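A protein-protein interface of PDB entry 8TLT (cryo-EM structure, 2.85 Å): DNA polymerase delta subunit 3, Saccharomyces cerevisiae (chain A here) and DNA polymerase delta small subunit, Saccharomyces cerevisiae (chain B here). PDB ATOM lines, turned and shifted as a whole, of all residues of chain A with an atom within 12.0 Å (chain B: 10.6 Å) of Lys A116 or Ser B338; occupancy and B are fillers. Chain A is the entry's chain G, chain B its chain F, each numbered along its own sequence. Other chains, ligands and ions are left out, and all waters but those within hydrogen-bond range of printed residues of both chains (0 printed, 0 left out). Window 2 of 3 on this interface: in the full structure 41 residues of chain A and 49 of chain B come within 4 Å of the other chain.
Of the printed residues of chain B, Lys A116 touches Asn B336 (3.7 Å) and Ser B338 (3.7 Å).
Of chain A, only Lys A116 comes within 4 Å of Ser B338.
No residue of chain B comes within 4 Å of Glu A114.
No residue of chain B comes within 4 Å of Val A117.
Ser A118 touches none of the printed residues of chain B.
Ser B333 touches none of the printed residues of chain A.
Of chain A, only Lys A116 comes within 4 Å of Asn B336.
No residue of chain A comes within 4 Å of Lys B340.
Printed residues of chain B within 4 Å of Ser A112: Arg B34.
Printed residues of chain A within 4 Å of Arg B34: Ser A112 (3.3 Å) and Tyr A113 (3.3 Å).
The nearest residue of chain A that does not touch Ser B338 is Ser A118 (4.7 Å).
The nearest printed residue of chain A that does not touch Tyr B334 is Lys A116 (6.2 Å).
The side-chain amide nitrogen (ND2) of Asn A111 is in hydrogen-bond range of the backbone carbonyl oxygen (O) of Tyr A113 (3.1 Å).
Printed residues of chain B that touch a printed residue of chain A: Arg B34, Tyr B334, Asn B336, Ser B338 and Glu B341.
Along chain A the printed residues that touch a printed residue of chain B span positions 112 to 116.
Among the printed residues, 6 pairs touch across the chains.
Ser A112 touches Arg B34 (CB to NH1, 3.3 Å).
Arg B34 touches Tyr A113 (NH2 to CE1, 3.3 Å).
Tyr A113 touches Glu B341 (CE1 to CG, 3.6 Å).
CD1 of Leu A115 touches CD1 of Tyr B334 (3.6 Å).
CG of Asn B336 touches O of Lys A116, at 3.7 Å.
Ser B338 touches Lys A116 (O to NZ, 3.7 Å).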
ATOM      1  N   ASN A 111      14.110  -4.058  -1.051  1.00  0.00           N
ATOM      2  CA  ASN A 111      14.390  -5.484  -1.049  1.00  0.00           C
ATOM      3  C   ASN A 111      15.893  -5.733  -0.971  1.00  0.00           C
ATOM      4  O   ASN A 111      16.714  -4.864  -1.276  1.00  0.00           O
ATOM      5  CB  ASN A 111      13.802  -6.163  -2.286  1.00  0.00           C
ATOM      6  CG  ASN A 111      14.416  -5.664  -3.573  1.00  0.00           C
ATOM      7  OD1 ASN A 111      14.915  -4.541  -3.643  1.00  0.00           O
ATOM      8  ND2 ASN A 111      14.379  -6.497  -4.606  1.00  0.00           N
ATOM      9  N   SER A 112      16.246  -6.947  -0.542  1.00  0.00           N
ATOM     10  CA  SER A 112      17.650  -7.288  -0.354  1.00  0.00           C
ATOM     11  C   SER A 112      18.412  -7.283  -1.674  1.00  0.00           C
ATOM     12  O   SER A 112      19.551  -6.808  -1.737  1.00  0.00           O
ATOM     13  CB  SER A 112      17.768  -8.649   0.330  1.00  0.00           C
ATOM     14  N   TYR A 113      17.803  -7.803  -2.734  1.00  0.00           N
ATOM     15  CA  TYR A 113      18.489  -7.939  -4.010  1.00  0.00           C
ATOM     16  C   TYR A 113      18.476  -6.626  -4.781  1.00  0.00           C
ATOM     17  O   TYR A 113      17.444  -5.958  -4.884  1.00  0.00           O
ATOM     18  CB  TYR A 113      17.841  -9.042  -4.845  1.00  0.00           C
ATOM     19  CG  TYR A 113      17.904 -10.402  -4.194  1.00  0.00           C
ATOM     20  CD1 TYR A 113      19.059 -11.168  -4.252  1.00  0.00           C
ATOM     21  CD2 TYR A 113      16.808 -10.918  -3.517  1.00  0.00           C
ATOM     22  CE1 TYR A 113      19.119 -12.411  -3.656  1.00  0.00           C
ATOM     23  CE2 TYR A 113      16.861 -12.159  -2.918  1.00  0.00           C
ATOM     24  CZ  TYR A 113      18.018 -12.901  -2.992  1.00  0.00           C
ATOM     25  OH  TYR A 113      18.075 -14.138  -2.397  1.00  0.00           O
ATOM     26  N   GLU A 114      19.632  -6.264  -5.326  1.00  0.00           N
ATOM     27  CA  GLU A 114      19.774  -5.069  -6.143  1.00  0.00           C
ATOM     28  C   GLU A 114      19.654  -5.427  -7.619  1.00  0.00           C
ATOM     29  O   GLU A 114      20.014  -6.529  -8.042  1.00  0.00           O
ATOM     30  CB  GLU A 114      21.116  -4.382  -5.879  1.00  0.00           C
ATOM     31  N   LEU A 115      19.149  -4.480  -8.401  1.00  0.00           N
ATOM     32  CA  LEU A 115      18.926  -4.706  -9.823  1.00  0.00           C
ATOM     33  C   LEU A 115      20.238  -4.583 -10.587  1.00  0.00           C
ATOM     34  O   LEU A 115      21.004  -3.638 -10.376  1.00  0.00           O
ATOM     35  CB  LEU A 115      17.899  -3.712 -10.362  1.00  0.00           C
ATOM     36  CG  LEU A 115      17.622  -3.746 -11.866  1.00  0.00           C
ATOM     37  CD1 LEU A 115      16.803  -4.971 -12.231  1.00  0.00           C
ATOM     38  CD2 LEU A 115      16.914  -2.476 -12.307  1.00  0.00           C
ATOM     39  N   LYS A 116      20.494  -5.540 -11.473  1.00  0.00           N
ATOM     40  CA  LYS A 116      21.689  -5.550 -12.306  1.00  0.00           C
ATOM     41  C   LYS A 116      21.291  -5.390 -13.767  1.00  0.00           C
ATOM     42  O   LYS A 116      20.389  -6.084 -14.248  1.00  0.00           O
ATOM     43  CB  LYS A 116      22.483  -6.843 -12.113  1.00  0.00           C
ATOM     44  CG  LYS A 116      22.363  -7.443 -10.723  1.00  0.00           C
ATOM     45  CD  LYS A 116      23.600  -8.249 -10.368  1.00  0.00           C
ATOM     46  CE  LYS A 116      23.242  -9.494  -9.577  1.00  0.00           C
ATOM     47  NZ  LYS A 116      23.067 -10.677 -10.462  1.00  0.00           N
ATOM     48  N   VAL A 117      21.964  -4.481 -14.465  1.00  0.00           N
ATOM     49  CA  VAL A 117      21.692  -4.191 -15.867  1.00  0.00           C
ATOM     50  C   VAL A 117      22.938  -4.518 -16.675  1.00  0.00           C
ATOM     51  O   VAL A 117      24.032  -4.037 -16.357  1.00  0.00           O
ATOM     52  CB  VAL A 117      21.274  -2.723 -16.075  1.00  0.00           C
ATOM     53  N   SER A 118      22.767  -5.334 -17.713  1.00  0.00           N
ATOM     54  CA  SER A 118      23.860  -5.744 -18.596  1.00  0.00           C
ATOM     55  C   SER A 118      25.011  -6.378 -17.821  1.00  0.00           C
ATOM     56  O   SER A 118      24.800  -7.022 -16.794  1.00  0.00           O
ATOM     57  CB  SER A 118      24.369  -4.550 -19.410  1.00  0.00           C
ATOM     58  N   ARG B  34      16.094 -11.479   3.479  1.00  0.00           N
ATOM     59  CA  ARG B  34      16.608 -12.195   2.318  1.00  0.00           C
ATOM     60  C   ARG B  34      16.073 -13.621   2.330  1.00  0.00           C
ATOM     61  O   ARG B  34      16.416 -14.414   3.213  1.00  0.00           O
ATOM     62  CB  ARG B  34      18.133 -12.181   2.316  1.00  0.00           C
ATOM     63  CG  ARG B  34      18.758 -12.731   1.046  1.00  0.00           C
ATOM     64  CD  ARG B  34      20.273 -12.650   1.100  1.00  0.00           C
ATOM     65  NE  ARG B  34      20.855 -12.376  -0.209  1.00  0.00           N
ATOM     66  CZ  ARG B  34      21.043 -11.161  -0.705  1.00  0.00           C
ATOM     67  NH1 ARG B  34      20.708 -10.078  -0.025  1.00  0.00           N
ATOM     68  NH2 ARG B  34      21.582 -11.031  -1.914  1.00  0.00           N
ATOM     69  N   LEU B  40      16.660 -22.240  -7.672  1.00  0.00           N
ATOM     70  CA  LEU B  40      16.675 -21.257  -8.751  1.00  0.00           C
ATOM     71  C   LEU B  40      17.652 -21.659  -9.847  1.00  0.00           C
ATOM     72  O   LEU B  40      17.293 -21.709 -11.029  1.00  0.00           O
ATOM     73  CB  LEU B  40      17.029 -19.879  -8.187  1.00  0.00           C
ATOM     74  CG  LEU B  40      16.372 -18.634  -8.788  1.00  0.00           C
ATOM     75  CD1 LEU B  40      16.836 -17.397  -8.041  1.00  0.00           C
ATOM     76  CD2 LEU B  40      16.657 -18.495 -10.275  1.00  0.00           C
ATOM     77  N   TYR B  41      18.897 -21.950  -9.475  1.00  0.00           N
ATOM     78  CA  TYR B  41      19.916 -22.364 -10.427  1.00  0.00           C
ATOM     79  C   TYR B  41      20.243 -23.846 -10.330  1.00  0.00           C
ATOM     80  O   TYR B  41      21.107 -24.326 -11.072  1.00  0.00           O
ATOM     81  CB  TYR B  41      21.188 -21.532 -10.233  1.00  0.00           C
ATOM     82  CG  TYR B  41      20.981 -20.055 -10.477  1.00  0.00           C
ATOM     83  CD1 TYR B  41      20.678 -19.578 -11.745  1.00  0.00           C
ATOM     84  CD2 TYR B  41      21.081 -19.139  -9.440  1.00  0.00           C
ATOM     85  CE1 TYR B  41      20.483 -18.230 -11.973  1.00  0.00           C
ATOM     86  CE2 TYR B  41      20.888 -17.789  -9.659  1.00  0.00           C
ATOM     87  CZ  TYR B  41      20.589 -17.340 -10.927  1.00  0.00           C
ATOM     88  OH  TYR B  41      20.396 -15.998 -11.150  1.00  0.00           O
ATOM     89  N   LYS B 324       8.556 -14.602 -21.922  1.00  0.00           N
ATOM     90  CA  LYS B 324       9.263 -13.364 -21.611  1.00  0.00           C
ATOM     91  C   LYS B 324       8.528 -12.151 -22.164  1.00  0.00           C
ATOM     92  O   LYS B 324       8.593 -11.064 -21.580  1.00  0.00           O
ATOM     93  CB  LYS B 324      10.687 -13.421 -22.161  1.00  0.00           C
ATOM     94  CG  LYS B 324      11.707 -13.960 -21.179  1.00  0.00           C
ATOM     95  CD  LYS B 324      13.064 -13.316 -21.387  1.00  0.00           C
ATOM     96  CE  LYS B 324      14.184 -14.250 -20.965  1.00  0.00           C
ATOM     97  NZ  LYS B 324      14.151 -15.530 -21.724  1.00  0.00           N
ATOM     98  N   SER B 330       8.806  -1.845 -19.619  1.00  0.00           N
ATOM     99  CA  SER B 330       9.485  -1.398 -18.410  1.00  0.00           C
ATOM    100  C   SER B 330      10.101  -2.544 -17.616  1.00  0.00           C
ATOM    101  O   SER B 330      10.850  -2.282 -16.669  1.00  0.00           O
ATOM    102  CB  SER B 330       8.510  -0.617 -17.528  1.00  0.00           C
ATOM    103  OG  SER B 330       7.547  -1.479 -16.947  1.00  0.00           O
ATOM    104  N   LEU B 331       9.810  -3.793 -17.971  1.00  0.00           N
ATOM    105  CA  LEU B 331      10.334  -4.959 -17.272  1.00  0.00           C
ATOM    106  C   LEU B 331      11.540  -5.572 -17.974  1.00  0.00           C
ATOM    107  O   LEU B 331      11.961  -6.678 -17.612  1.00  0.00           O
ATOM    108  CB  LEU B 331       9.231  -6.009 -17.110  1.00  0.00           C
ATOM    109  CG  LEU B 331       8.485  -6.043 -15.774  1.00  0.00           C
ATOM    110  CD1 LEU B 331       7.827  -4.709 -15.484  1.00  0.00           C
ATOM    111  CD2 LEU B 331       7.453  -7.156 -15.771  1.00  0.00           C
ATOM    112  N   GLU B 332      12.105  -4.880 -18.967  1.00  0.00           N
ATOM    113  CA  GLU B 332      13.239  -5.426 -19.705  1.00  0.00           C
ATOM    114  C   GLU B 332      14.444  -5.635 -18.798  1.00  0.00           C
ATOM    115  O   GLU B 332      15.168  -6.627 -18.936  1.00  0.00           O
ATOM    116  CB  GLU B 332      13.601  -4.505 -20.870  1.00  0.00           C
ATOM    117  CG  GLU B 332      12.661  -4.604 -22.057  1.00  0.00           C
ATOM    118  N   SER B 333      14.681  -4.707 -17.868  1.00  0.00           N
ATOM    119  CA  SER B 333      15.792  -4.864 -16.937  1.00  0.00           C
ATOM    120  C   SER B 333      15.607  -6.100 -16.067  1.00  0.00           C
ATOM    121  O   SER B 333      16.567  -6.833 -15.803  1.00  0.00           O
ATOM    122  CB  SER B 333      15.934  -3.613 -16.072  1.00  0.00           C
ATOM    123  N   TYR B 334      14.378  -6.345 -15.609  1.00  0.00           N
ATOM    124  CA  TYR B 334      14.110  -7.530 -14.804  1.00  0.00           C
ATOM    125  C   TYR B 334      14.202  -8.804 -15.630  1.00  0.00           C
ATOM    126  O   TYR B 334      14.486  -9.876 -15.084  1.00  0.00           O
ATOM    127  CB  TYR B 334      12.735  -7.414 -14.152  1.00  0.00           C
ATOM    128  CG  TYR B 334      12.628  -6.263 -13.181  1.00  0.00           C
ATOM    129  CD1 TYR B 334      13.397  -6.233 -12.027  1.00  0.00           C
ATOM    130  CD2 TYR B 334      11.775  -5.197 -13.428  1.00  0.00           C
ATOM    131  CE1 TYR B 334      13.308  -5.181 -11.140  1.00  0.00           C
ATOM    132  CE2 TYR B 334      11.680  -4.141 -12.547  1.00  0.00           C
ATOM    133  CZ  TYR B 334      12.449  -4.138 -11.404  1.00  0.00           C
ATOM    134  OH  TYR B 334      12.358  -3.088 -10.523  1.00  0.00           O
ATOM    135  N   PHE B 335      13.965  -8.713 -16.938  1.00  0.00           N
ATOM    136  CA  PHE B 335      14.036  -9.870 -17.821  1.00  0.00           C
ATOM    137  C   PHE B 335      15.383  -9.984 -18.528  1.00  0.00           C
ATOM    138  O   PHE B 335      15.490 -10.693 -19.533  1.00  0.00           O
ATOM    139  CB  PHE B 335      12.902  -9.824 -18.845  1.00  0.00           C
ATOM    140  CG  PHE B 335      11.558 -10.169 -18.272  1.00  0.00           C
ATOM    141  CD1 PHE B 335      11.383 -11.327 -17.537  1.00  0.00           C
ATOM    142  CD2 PHE B 335      10.474  -9.333 -18.465  1.00  0.00           C
ATOM    143  CE1 PHE B 335      10.150 -11.646 -17.007  1.00  0.00           C
ATOM    144  CE2 PHE B 335       9.239  -9.647 -17.936  1.00  0.00           C
ATOM    145  CZ  PHE B 335       9.078 -10.806 -17.207  1.00  0.00           C
ATOM    146  N   ASN B 336      16.415  -9.304 -18.020  1.00  0.00           N
ATOM    147  CA  ASN B 336      17.734  -9.375 -18.639  1.00  0.00           C
ATOM    148  C   ASN B 336      18.362 -10.756 -18.512  1.00  0.00           C
ATOM    149  O   ASN B 336      19.241 -11.098 -19.310  1.00  0.00           O
ATOM    150  CB  ASN B 336      18.664  -8.327 -18.027  1.00  0.00           C
ATOM    151  CG  ASN B 336      18.992  -8.617 -16.576  1.00  0.00           C
ATOM    152  N   GLY B 337      17.939 -11.551 -17.533  1.00  0.00           N
ATOM    153  CA  GLY B 337      18.458 -12.895 -17.374  1.00  0.00           C
ATOM    154  C   GLY B 337      19.283 -13.077 -16.118  1.00  0.00           C
ATOM    155  O   GLY B 337      19.188 -14.110 -15.449  1.00  0.00           O
ATOM    156  N   SER B 338      20.099 -12.076 -15.788  1.00  0.00           N
ATOM    157  CA  SER B 338      20.950 -12.171 -14.608  1.00  0.00           C
ATOM    158  C   SER B 338      20.174 -11.952 -13.315  1.00  0.00           C
ATOM    159  O   SER B 338      20.511 -12.552 -12.289  1.00  0.00           O
ATOM    160  CB  SER B 338      22.096 -11.164 -14.704  1.00  0.00           C
ATOM    161  OG  SER B 338      21.601  -9.849 -14.889  1.00  0.00           O
ATOM    162  N   ASN B 339      19.147 -11.103 -13.339  1.00  0.00           N
ATOM    163  CA  ASN B 339      18.387 -10.763 -12.136  1.00  0.00           C
ATOM    164  C   ASN B 339      17.108 -11.595 -12.102  1.00  0.00           C
ATOM    165  O   ASN B 339      16.012 -11.121 -12.399  1.00  0.00           O
ATOM    166  CB  ASN B 339      18.090  -9.266 -12.098  1.00  0.00           C
ATOM    167  N   LYS B 340      17.260 -12.863 -11.722  1.00  0.00           N
ATOM    168  CA  LYS B 340      16.128 -13.757 -11.522  1.00  0.00           C
ATOM    169  C   LYS B 340      15.744 -13.903 -10.058  1.00  0.00           C
ATOM    170  O   LYS B 340      14.796 -14.630  -9.748  1.00  0.00           O
ATOM    171  CB  LYS B 340      16.425 -15.138 -12.117  1.00  0.00           C
ATOM    172  CG  LYS B 340      15.634 -15.448 -13.377  1.00  0.00           C
ATOM    173  CD  LYS B 340      15.838 -16.885 -13.828  1.00  0.00           C
ATOM    174  CE  LYS B 340      17.183 -17.070 -14.507  1.00  0.00           C
ATOM    175  NZ  LYS B 340      17.111 -18.070 -15.606  1.00  0.00           N
ATOM    176  N   GLU B 341      16.459 -13.237  -9.151  1.00  0.00           N
ATOM    177  CA  GLU B 341      16.096 -13.256  -7.741  1.00  0.00           C
ATOM    178  C   GLU B 341      14.986 -12.269  -7.411  1.00  0.00           C
ATOM    179  O   GLU B 341      14.344 -12.406  -6.365  1.00  0.00           O
ATOM    180  CB  GLU B 341      17.321 -12.960  -6.875  1.00  0.00           C
ATOM    181  CG  GLU B 341      18.202 -14.167  -6.616  1.00  0.00           C
ATOM    182  CD  GLU B 341      19.259 -14.356  -7.683  1.00  0.00           C
ATOM    183  OE1 GLU B 341      20.163 -15.192  -7.480  1.00  0.00           O
ATOM    184  OE2 GLU B 341      19.191 -13.667  -8.721  1.00  0.00           O
ATOM    185  N   ILE B 342      14.751 -11.281  -8.269  1.00  0.00           N
ATOM    186  CA  ILE B 342      13.669 -10.324  -8.060  1.00  0.00           C
ATOM    187  C   ILE B 342      12.380 -10.798  -8.715  1.00  0.00           C
ATOM    188  O   ILE B 342      11.329 -10.856  -8.072  1.00  0.00           O
ATOM    189  CB  ILE B 342      14.086  -8.930  -8.577  1.00  0.00           C
ATOM    190  N   LEU B 343      12.436 -11.143  -9.998  1.00  0.00           N
ATOM    191  CA  LEU B 343      11.295 -11.679 -10.724  1.00  0.00           C
ATOM    192  C   LEU B 343      11.651 -13.057 -11.258  1.00  0.00           C
ATOM    193  O   LEU B 343      12.665 -13.217 -11.946  1.00  0.00           O
ATOM    194  CB  LEU B 343      10.884 -10.757 -11.874  1.00  0.00           C
ATOM    195  CG  LEU B 343       9.585 -11.123 -12.591  1.00  0.00           C
ATOM    196  CD1 LEU B 343       8.445 -11.244 -11.598  1.00  0.00           C
ATOM    197  CD2 LEU B 343       9.259 -10.100 -13.663  1.00  0.00           C
ATOM    198  N   ASN B 344      10.819 -14.047 -10.945  1.00  0.00           N
ATOM    199  CA  ASN B 344      11.045 -15.420 -11.370  1.00  0.00           C
ATOM    200  C   ASN B 344       9.748 -15.996 -11.914  1.00  0.00           C
ATOM    201  O   ASN B 344       8.705 -15.915 -11.258  1.00  0.00           O
ATOM    202  CB  ASN B 344      11.566 -16.275 -10.210  1.00  0.00           C
ATOM    203  CG  ASN B 344      12.091 -17.618 -10.668  1.00  0.00           C
ATOM    204  OD1 ASN B 344      12.500 -17.778 -11.816  1.00  0.00           O
ATOM    205  ND2 ASN B 344      12.085 -18.594  -9.768  1.00  0.00           N
